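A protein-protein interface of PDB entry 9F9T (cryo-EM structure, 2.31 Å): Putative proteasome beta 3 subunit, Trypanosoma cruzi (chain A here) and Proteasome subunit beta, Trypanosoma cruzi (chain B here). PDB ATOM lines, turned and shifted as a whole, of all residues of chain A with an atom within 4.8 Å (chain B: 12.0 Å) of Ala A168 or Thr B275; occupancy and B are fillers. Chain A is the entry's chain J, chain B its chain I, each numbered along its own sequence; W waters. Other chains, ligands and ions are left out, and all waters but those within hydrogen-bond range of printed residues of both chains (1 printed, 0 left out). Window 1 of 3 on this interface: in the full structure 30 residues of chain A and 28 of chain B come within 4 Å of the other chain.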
ATOM      1  N   PHE A 164     -23.015   4.476 -21.117  1.00  0.00           N
ATOM      2  CA  PHE A 164     -22.519   5.538 -21.924  1.00  0.00           C
ATOM      3  C   PHE A 164     -21.402   6.327 -21.244  1.00  0.00           C
ATOM      4  O   PHE A 164     -20.451   6.725 -21.934  1.00  0.00           O
ATOM      5  CB  PHE A 164     -23.636   6.494 -22.257  1.00  0.00           C
ATOM      6  CG  PHE A 164     -23.132   7.757 -22.895  1.00  0.00           C
ATOM      7  CD1 PHE A 164     -22.725   7.765 -24.225  1.00  0.00           C
ATOM      8  CD2 PHE A 164     -22.976   8.909 -22.133  1.00  0.00           C
ATOM      9  CE1 PHE A 164     -22.174   8.910 -24.780  1.00  0.00           C
ATOM     10  CE2 PHE A 164     -22.515  10.070 -22.725  1.00  0.00           C
ATOM     11  CZ  PHE A 164     -22.085  10.056 -24.043  1.00  0.00           C
ATOM     12  N   GLU A 165     -21.476   6.583 -19.921  1.00  0.00           N
ATOM     13  CA  GLU A 165     -20.411   7.354 -19.255  1.00  0.00           C
ATOM     14  C   GLU A 165     -19.154   6.516 -19.201  1.00  0.00           C
ATOM     15  O   GLU A 165     -18.104   7.014 -19.560  1.00  0.00           O
ATOM     16  CB  GLU A 165     -20.706   7.800 -17.831  1.00  0.00           C
ATOM     17  CG  GLU A 165     -22.029   8.502 -17.717  1.00  0.00           C
ATOM     18  CD  GLU A 165     -22.150   9.759 -18.542  1.00  0.00           C
ATOM     19  OE1 GLU A 165     -23.213  10.003 -19.156  1.00  0.00           O
ATOM     20  OE2 GLU A 165     -21.180  10.495 -18.562  1.00  0.00           O
ATOM     21  N   VAL A 166     -19.276   5.268 -18.753  1.00  0.00           N
ATOM     22  CA  VAL A 166     -18.116   4.420 -18.721  1.00  0.00           C
ATOM     23  C   VAL A 166     -17.383   4.559 -20.052  1.00  0.00           C
ATOM     24  O   VAL A 166     -16.169   4.799 -20.086  1.00  0.00           O
ATOM     25  CB  VAL A 166     -18.474   2.946 -18.406  1.00  0.00           C
ATOM     26  CG1 VAL A 166     -17.365   1.936 -18.779  1.00  0.00           C
ATOM     27  CG2 VAL A 166     -18.772   2.792 -16.933  1.00  0.00           C
ATOM     28  N   ALA A 167     -18.149   4.390 -21.161  1.00  0.00           N
ATOM     29  CA  ALA A 167     -17.587   4.209 -22.496  1.00  0.00           C
ATOM     30  C   ALA A 167     -17.057   5.519 -23.089  1.00  0.00           C
ATOM     31  O   ALA A 167     -16.065   5.475 -23.798  1.00  0.00           O
ATOM     32  CB  ALA A 167     -18.588   3.558 -23.368  1.00  0.00           C
ATOM     33  N   ALA A 168     -17.582   6.666 -22.665  1.00  0.00           N
ATOM     34  CA  ALA A 168     -17.044   7.957 -23.057  1.00  0.00           C
ATOM     35  C   ALA A 168     -15.816   8.363 -22.222  1.00  0.00           C
ATOM     36  O   ALA A 168     -14.825   8.869 -22.747  1.00  0.00           O
ATOM     37  CB  ALA A 168     -18.139   8.972 -22.923  1.00  0.00           C
ATOM     38  N   GLN A 169     -15.824   8.127 -20.906  1.00  0.00           N
ATOM     39  CA  GLN A 169     -14.617   8.383 -20.146  1.00  0.00           C
ATOM     40  C   GLN A 169     -13.490   7.522 -20.649  1.00  0.00           C
ATOM     41  O   GLN A 169     -12.387   8.009 -20.733  1.00  0.00           O
ATOM     42  CB  GLN A 169     -14.770   8.113 -18.658  1.00  0.00           C
ATOM     43  CG  GLN A 169     -15.741   9.090 -18.051  1.00  0.00           C
ATOM     44  CD  GLN A 169     -15.234  10.503 -18.180  1.00  0.00           C
ATOM     45  OE1 GLN A 169     -14.074  10.819 -17.885  1.00  0.00           O
ATOM     46  NE2 GLN A 169     -16.116  11.393 -18.602  1.00  0.00           N
ATOM     47  N   ALA A 170     -13.775   6.284 -21.039  1.00  0.00           N
ATOM     48  CA  ALA A 170     -12.721   5.410 -21.533  1.00  0.00           C
ATOM     49  C   ALA A 170     -12.069   5.998 -22.776  1.00  0.00           C
ATOM     50  O   ALA A 170     -10.871   6.220 -22.810  1.00  0.00           O
ATOM     51  CB  ALA A 170     -13.259   4.026 -21.869  1.00  0.00           C
ATOM     52  N   MET A 171     -12.900   6.261 -23.779  1.00  0.00           N
ATOM     53  CA  MET A 171     -12.399   6.705 -25.059  1.00  0.00           C
ATOM     54  C   MET A 171     -11.632   8.006 -24.844  1.00  0.00           C
ATOM     55  O   MET A 171     -10.433   8.043 -25.170  1.00  0.00           O
ATOM     56  CB  MET A 171     -13.507   6.827 -26.084  1.00  0.00           C
ATOM     57  CG  MET A 171     -13.036   7.285 -27.448  1.00  0.00           C
ATOM     58  SD  MET A 171     -11.690   6.275 -28.085  1.00  0.00           S
ATOM     59  CE  MET A 171     -12.602   4.836 -28.628  1.00  0.00           C
ATOM     60  N   LEU A 172     -12.185   8.972 -24.101  1.00  0.00           N
ATOM     61  CA  LEU A 172     -11.426  10.215 -23.918  1.00  0.00           C
ATOM     62  C   LEU A 172     -10.057  10.042 -23.206  1.00  0.00           C
ATOM     63  O   LEU A 172      -9.013  10.461 -23.694  1.00  0.00           O
ATOM     64  CB  LEU A 172     -12.287  11.236 -23.200  1.00  0.00           C
ATOM     65  CG  LEU A 172     -13.547  11.601 -23.963  1.00  0.00           C
ATOM     66  CD1 LEU A 172     -14.424  12.535 -23.165  1.00  0.00           C
ATOM     67  CD2 LEU A 172     -13.223  12.165 -25.340  1.00  0.00           C
ATOM     68  N   ILE A 200     -19.443  13.674 -28.453  1.00  0.00           N
ATOM     69  CA  ILE A 200     -18.816  14.002 -27.181  1.00  0.00           C
ATOM     70  C   ILE A 200     -17.693  14.994 -27.399  1.00  0.00           C
ATOM     71  O   ILE A 200     -16.896  14.787 -28.285  1.00  0.00           O
ATOM     72  CB  ILE A 200     -18.203  12.706 -26.638  1.00  0.00           C
ATOM     73  CG1 ILE A 200     -19.256  11.610 -26.557  1.00  0.00           C
ATOM     74  CG2 ILE A 200     -17.456  12.912 -25.327  1.00  0.00           C
ATOM     75  CD1 ILE A 200     -18.620  10.269 -26.228  1.00  0.00           C
ATOM     76  N   ILE B 268     -16.445   1.854  -9.166  1.00  0.00           N
ATOM     77  CA  ILE B 268     -16.260   3.256  -9.499  1.00  0.00           C
ATOM     78  C   ILE B 268     -17.478   3.689 -10.295  1.00  0.00           C
ATOM     79  O   ILE B 268     -17.819   3.006 -11.254  1.00  0.00           O
ATOM     80  CB  ILE B 268     -14.967   3.457 -10.314  1.00  0.00           C
ATOM     81  CG1 ILE B 268     -13.761   2.830  -9.606  1.00  0.00           C
ATOM     82  CG2 ILE B 268     -14.753   4.926 -10.642  1.00  0.00           C
ATOM     83  CD1 ILE B 268     -12.508   2.775 -10.432  1.00  0.00           C
ATOM     84  N   ARG B 269     -18.103   4.799  -9.875  1.00  0.00           N
ATOM     85  CA  ARG B 269     -19.383   5.245 -10.409  1.00  0.00           C
ATOM     86  C   ARG B 269     -19.206   6.567 -11.138  1.00  0.00           C
ATOM     87  O   ARG B 269     -18.497   7.449 -10.667  1.00  0.00           O
ATOM     88  CB  ARG B 269     -20.427   5.513  -9.315  1.00  0.00           C
ATOM     89  CG  ARG B 269     -20.674   4.364  -8.348  1.00  0.00           C
ATOM     90  CD  ARG B 269     -20.906   3.048  -9.066  1.00  0.00           C
ATOM     91  NE  ARG B 269     -21.515   2.024  -8.217  1.00  0.00           N
ATOM     92  CZ  ARG B 269     -22.801   1.985  -7.868  1.00  0.00           C
ATOM     93  NH1 ARG B 269     -23.611   2.982  -8.188  1.00  0.00           N
ATOM     94  NH2 ARG B 269     -23.268   0.942  -7.200  1.00  0.00           N
ATOM     95  N   PHE B 270     -19.896   6.690 -12.274  1.00  0.00           N
ATOM     96  CA  PHE B 270     -20.122   7.978 -12.894  1.00  0.00           C
ATOM     97  C   PHE B 270     -21.625   8.243 -12.875  1.00  0.00           C
ATOM     98  O   PHE B 270     -22.369   7.546 -13.563  1.00  0.00           O
ATOM     99  CB  PHE B 270     -19.481   8.030 -14.288  1.00  0.00           C
ATOM    100  CG  PHE B 270     -17.975   7.911 -14.282  1.00  0.00           C
ATOM    101  CD1 PHE B 270     -17.202   8.631 -13.368  1.00  0.00           C
ATOM    102  CD2 PHE B 270     -17.322   7.070 -15.174  1.00  0.00           C
ATOM    103  CE1 PHE B 270     -15.822   8.492 -13.322  1.00  0.00           C
ATOM    104  CE2 PHE B 270     -15.935   6.955 -15.142  1.00  0.00           C
ATOM    105  CZ  PHE B 270     -15.188   7.668 -14.222  1.00  0.00           C
ATOM    106  N   PRO B 271     -22.098   9.242 -12.082  1.00  0.00           N
ATOM    107  CA  PRO B 271     -23.462   9.764 -12.219  1.00  0.00           C
ATOM    108  C   PRO B 271     -23.756  10.250 -13.644  1.00  0.00           C
ATOM    109  O   PRO B 271     -23.082  11.153 -14.128  1.00  0.00           O
ATOM    110  CB  PRO B 271     -23.534  10.966 -11.249  1.00  0.00           C
ATOM    111  CG  PRO B 271     -22.101  11.219 -10.767  1.00  0.00           C
ATOM    112  CD  PRO B 271     -21.329   9.947 -11.044  1.00  0.00           C
ATOM    113  N   PRO B 272     -24.760   9.686 -14.360  1.00  0.00           N
ATOM    114  CA  PRO B 272     -25.176  10.184 -15.680  1.00  0.00           C
ATOM    115  C   PRO B 272     -25.258  11.705 -15.865  1.00  0.00           C
ATOM    116  O   PRO B 272     -25.958  12.379 -15.111  1.00  0.00           O
ATOM    117  CB  PRO B 272     -26.589   9.584 -15.811  1.00  0.00           C
ATOM    118  CG  PRO B 272     -26.497   8.263 -15.088  1.00  0.00           C
ATOM    119  CD  PRO B 272     -25.556   8.526 -13.930  1.00  0.00           C
ATOM    120  N   GLY B 273     -24.561  12.230 -16.895  1.00  0.00           N
ATOM    121  CA  GLY B 273     -24.280  13.659 -17.023  1.00  0.00           C
ATOM    122  C   GLY B 273     -22.879  14.068 -16.536  1.00  0.00           C
ATOM    123  O   GLY B 273     -22.629  15.241 -16.280  1.00  0.00           O
ATOM    124  N   THR B 274     -21.956  13.099 -16.480  1.00  0.00           N
ATOM    125  CA  THR B 274     -20.563  13.273 -16.080  1.00  0.00           C
ATOM    126  C   THR B 274     -19.747  13.753 -17.298  1.00  0.00           C
ATOM    127  O   THR B 274     -18.881  14.635 -17.175  1.00  0.00           O
ATOM    128  CB  THR B 274     -20.084  11.979 -15.390  1.00  0.00           C
ATOM    129  OG1 THR B 274     -20.391  12.004 -13.994  1.00  0.00           O
ATOM    130  CG2 THR B 274     -18.597  11.727 -15.491  1.00  0.00           C
ATOM    131  N   THR B 275     -20.100  13.230 -18.490  1.00  0.00           N
ATOM    132  CA  THR B 275     -19.438  13.515 -19.757  1.00  0.00           C
ATOM    133  C   THR B 275     -20.187  14.636 -20.503  1.00  0.00           C
ATOM    134  O   THR B 275     -21.384  14.548 -20.724  1.00  0.00           O
ATOM    135  CB  THR B 275     -19.252  12.192 -20.528  1.00  0.00           C
ATOM    136  OG1 THR B 275     -18.577  11.263 -19.668  1.00  0.00           O
ATOM    137  CG2 THR B 275     -18.456  12.336 -21.813  1.00  0.00           C
ATOM    138  N   PRO B 276     -19.531  15.778 -20.850  1.00  0.00           N
ATOM    139  CA  PRO B 276     -20.113  16.812 -21.714  1.00  0.00           C
ATOM    140  C   PRO B 276     -20.407  16.443 -23.176  1.00  0.00           C
ATOM    141  O   PRO B 276     -19.508  16.215 -23.979  1.00  0.00           O
ATOM    142  CB  PRO B 276     -19.041  17.921 -21.724  1.00  0.00           C
ATOM    143  CG  PRO B 276     -18.308  17.720 -20.425  1.00  0.00           C
ATOM    144  CD  PRO B 276     -18.225  16.218 -20.332  1.00  0.00           C
ATOM    145  N   VAL B 277     -21.689  16.460 -23.520  1.00  0.00           N
ATOM    146  CA  VAL B 277     -22.134  16.156 -24.869  1.00  0.00           C
ATOM    147  C   VAL B 277     -22.405  17.476 -25.605  1.00  0.00           C
ATOM    148  O   VAL B 277     -22.999  18.418 -25.070  1.00  0.00           O
ATOM    149  CB  VAL B 277     -23.335  15.200 -24.756  1.00  0.00           C
ATOM    150  CG1 VAL B 277     -24.149  15.089 -26.022  1.00  0.00           C
ATOM    151  CG2 VAL B 277     -22.879  13.830 -24.279  1.00  0.00           C
ATOM    152  N   LEU B 278     -21.923  17.556 -26.848  1.00  0.00           N
ATOM    153  CA  LEU B 278     -22.167  18.720 -27.680  1.00  0.00           C
ATOM    154  C   LEU B 278     -23.519  18.553 -28.337  1.00  0.00           C
ATOM    155  O   LEU B 278     -24.197  19.553 -28.533  1.00  0.00           O
ATOM    156  CB  LEU B 278     -21.064  18.898 -28.738  1.00  0.00           C
ATOM    157  CG  LEU B 278     -19.681  19.277 -28.197  1.00  0.00           C
ATOM    158  CD1 LEU B 278     -18.624  19.233 -29.297  1.00  0.00           C
ATOM    159  CD2 LEU B 278     -19.703  20.647 -27.512  1.00  0.00           C
ATOM    160  N   ARG B 279     -23.867  17.318 -28.712  1.00  0.00           N
ATOM    161  CA  ARG B 279     -24.969  17.083 -29.635  1.00  0.00           C
ATOM    162  C   ARG B 279     -25.506  15.662 -29.505  1.00  0.00           C
ATOM    163  O   ARG B 279     -24.758  14.715 -29.320  1.00  0.00           O
ATOM    164  CB  ARG B 279     -24.519  17.368 -31.066  1.00  0.00           C
ATOM    165  CG  ARG B 279     -24.848  18.769 -31.563  1.00  0.00           C
ATOM    166  CD  ARG B 279     -24.317  19.024 -32.972  1.00  0.00           C
ATOM    167  NE  ARG B 279     -25.173  18.441 -34.008  1.00  0.00           N
ATOM    168  CZ  ARG B 279     -24.792  18.179 -35.261  1.00  0.00           C
ATOM    169  NH1 ARG B 279     -25.693  17.839 -36.168  1.00  0.00           N
ATOM    170  NH2 ARG B 279     -23.520  18.297 -35.614  1.00  0.00           N
ATOM    171  N   GLU B 280     -26.824  15.527 -29.672  1.00  0.00           N
ATOM    172  CA  GLU B 280     -27.531  14.277 -29.425  1.00  0.00           C
ATOM    173  C   GLU B 280     -28.553  14.080 -30.537  1.00  0.00           C
ATOM    174  O   GLU B 280     -29.187  15.042 -30.949  1.00  0.00           O
ATOM    175  CB  GLU B 280     -28.180  14.337 -28.033  1.00  0.00           C
ATOM    176  CG  GLU B 280     -28.961  13.084 -27.636  1.00  0.00           C
ATOM    177  CD  GLU B 280     -29.283  12.916 -26.146  1.00  0.00           C
ATOM    178  OE1 GLU B 280     -28.352  13.016 -25.296  1.00  0.00           O
ATOM    179  OE2 GLU B 280     -30.465  12.642 -25.826  1.00  0.00           O
HETATM  180  O   HOH W   1     -23.043  12.345 -20.198  1.00  0.00           O
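The backbone NH (N) of Thr B274 sits at hydrogen-bond distance from the side-chain carboxylate (OE2) of Glu A165 (3.4 Å). The side-chain amide nitrogen (NE2) of Gln A169 lies within hydrogen-bond range of the side-chain hydroxyl (OG1) of Thr B275 (2.7 Å). The side-chain hydroxyl (OG1) of Thr B275 sits at hydrogen-bond distance from the side-chain carboxylate (OE2) of Glu A165, at 2.9 Å. The side-chain carboxylate (OE1) of Glu A165 sits at hydrogen-bond distance from the backbone NH (N) of Gly B273 (3.4 Å).
The side-chain hydroxyl (OG1) of Thr B274 lies within hydrogen-bond range of the backbone carbonyl oxygen (O) of Pro B271 (2.8 Å).
Among the printed residues, merely in contact across the chains: Phe A164 with Val B277 (3.9 Å), Glu A165 with Phe B270 (3.8 Å), Glu A165 with Pro B272 (3.996 Å), Ala A168 with Thr B275 (3.6 Å), Gln A169 with Phe B270 (3.6 Å), Gln A169 with Thr B274 (3.99 Å), Ile A200 with Thr B275 (3.7 Å) and Ile A200 with Pro B276 (3.95 Å).
Ala A168 touches just one residue of chain B: Thr B275. Thr B275 touches just these residues of chain A: Glu A165, Ala A168, Gln A169 and Ile A200. Val A166 touches none of the printed residues of chain B. No residue of chain B comes within 4 Å of Ala A167. Ala A170 touches none of the printed residues of chain B. No residue of chain B comes within 4 Å of Met A171. No residue of chain B comes within 4 Å of Leu A172. Ile A200 touches just these residues of chain B: Thr B275 (3.7 Å) and Pro B276 (3.95 Å). Of the printed residues of chain A, Pro B272 touches Glu A165 (3.996 Å). Of the printed residues of chain A, Pro B276 touches Ile A200 (3.95 Å). Printed residues of chain A within 4 Å of Thr B274: Glu A165 and Gln A169. Of the printed residues of chain A, Phe B270 touches Glu A165 and Gln A169.
Hydrophobic or aromatic side chains of chain A within 4 Å of the printed part of chain B: Phe A164, Ala A168 and Ile A200. Of the 13 printed residues of chain B, 7 touch a printed residue of chain A. Among the printed residues, 12 pairs touch across the chains. Among the printed residues, no Asp or Glu carboxylate lies within 4 Å of a Lys or Arg side-chain nitrogen of the other chain.
Water W1 lies within hydrogen-bond range of OE1 of Glu A165 (2.6 Å) and O of Thr B275 (2.8 Å).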
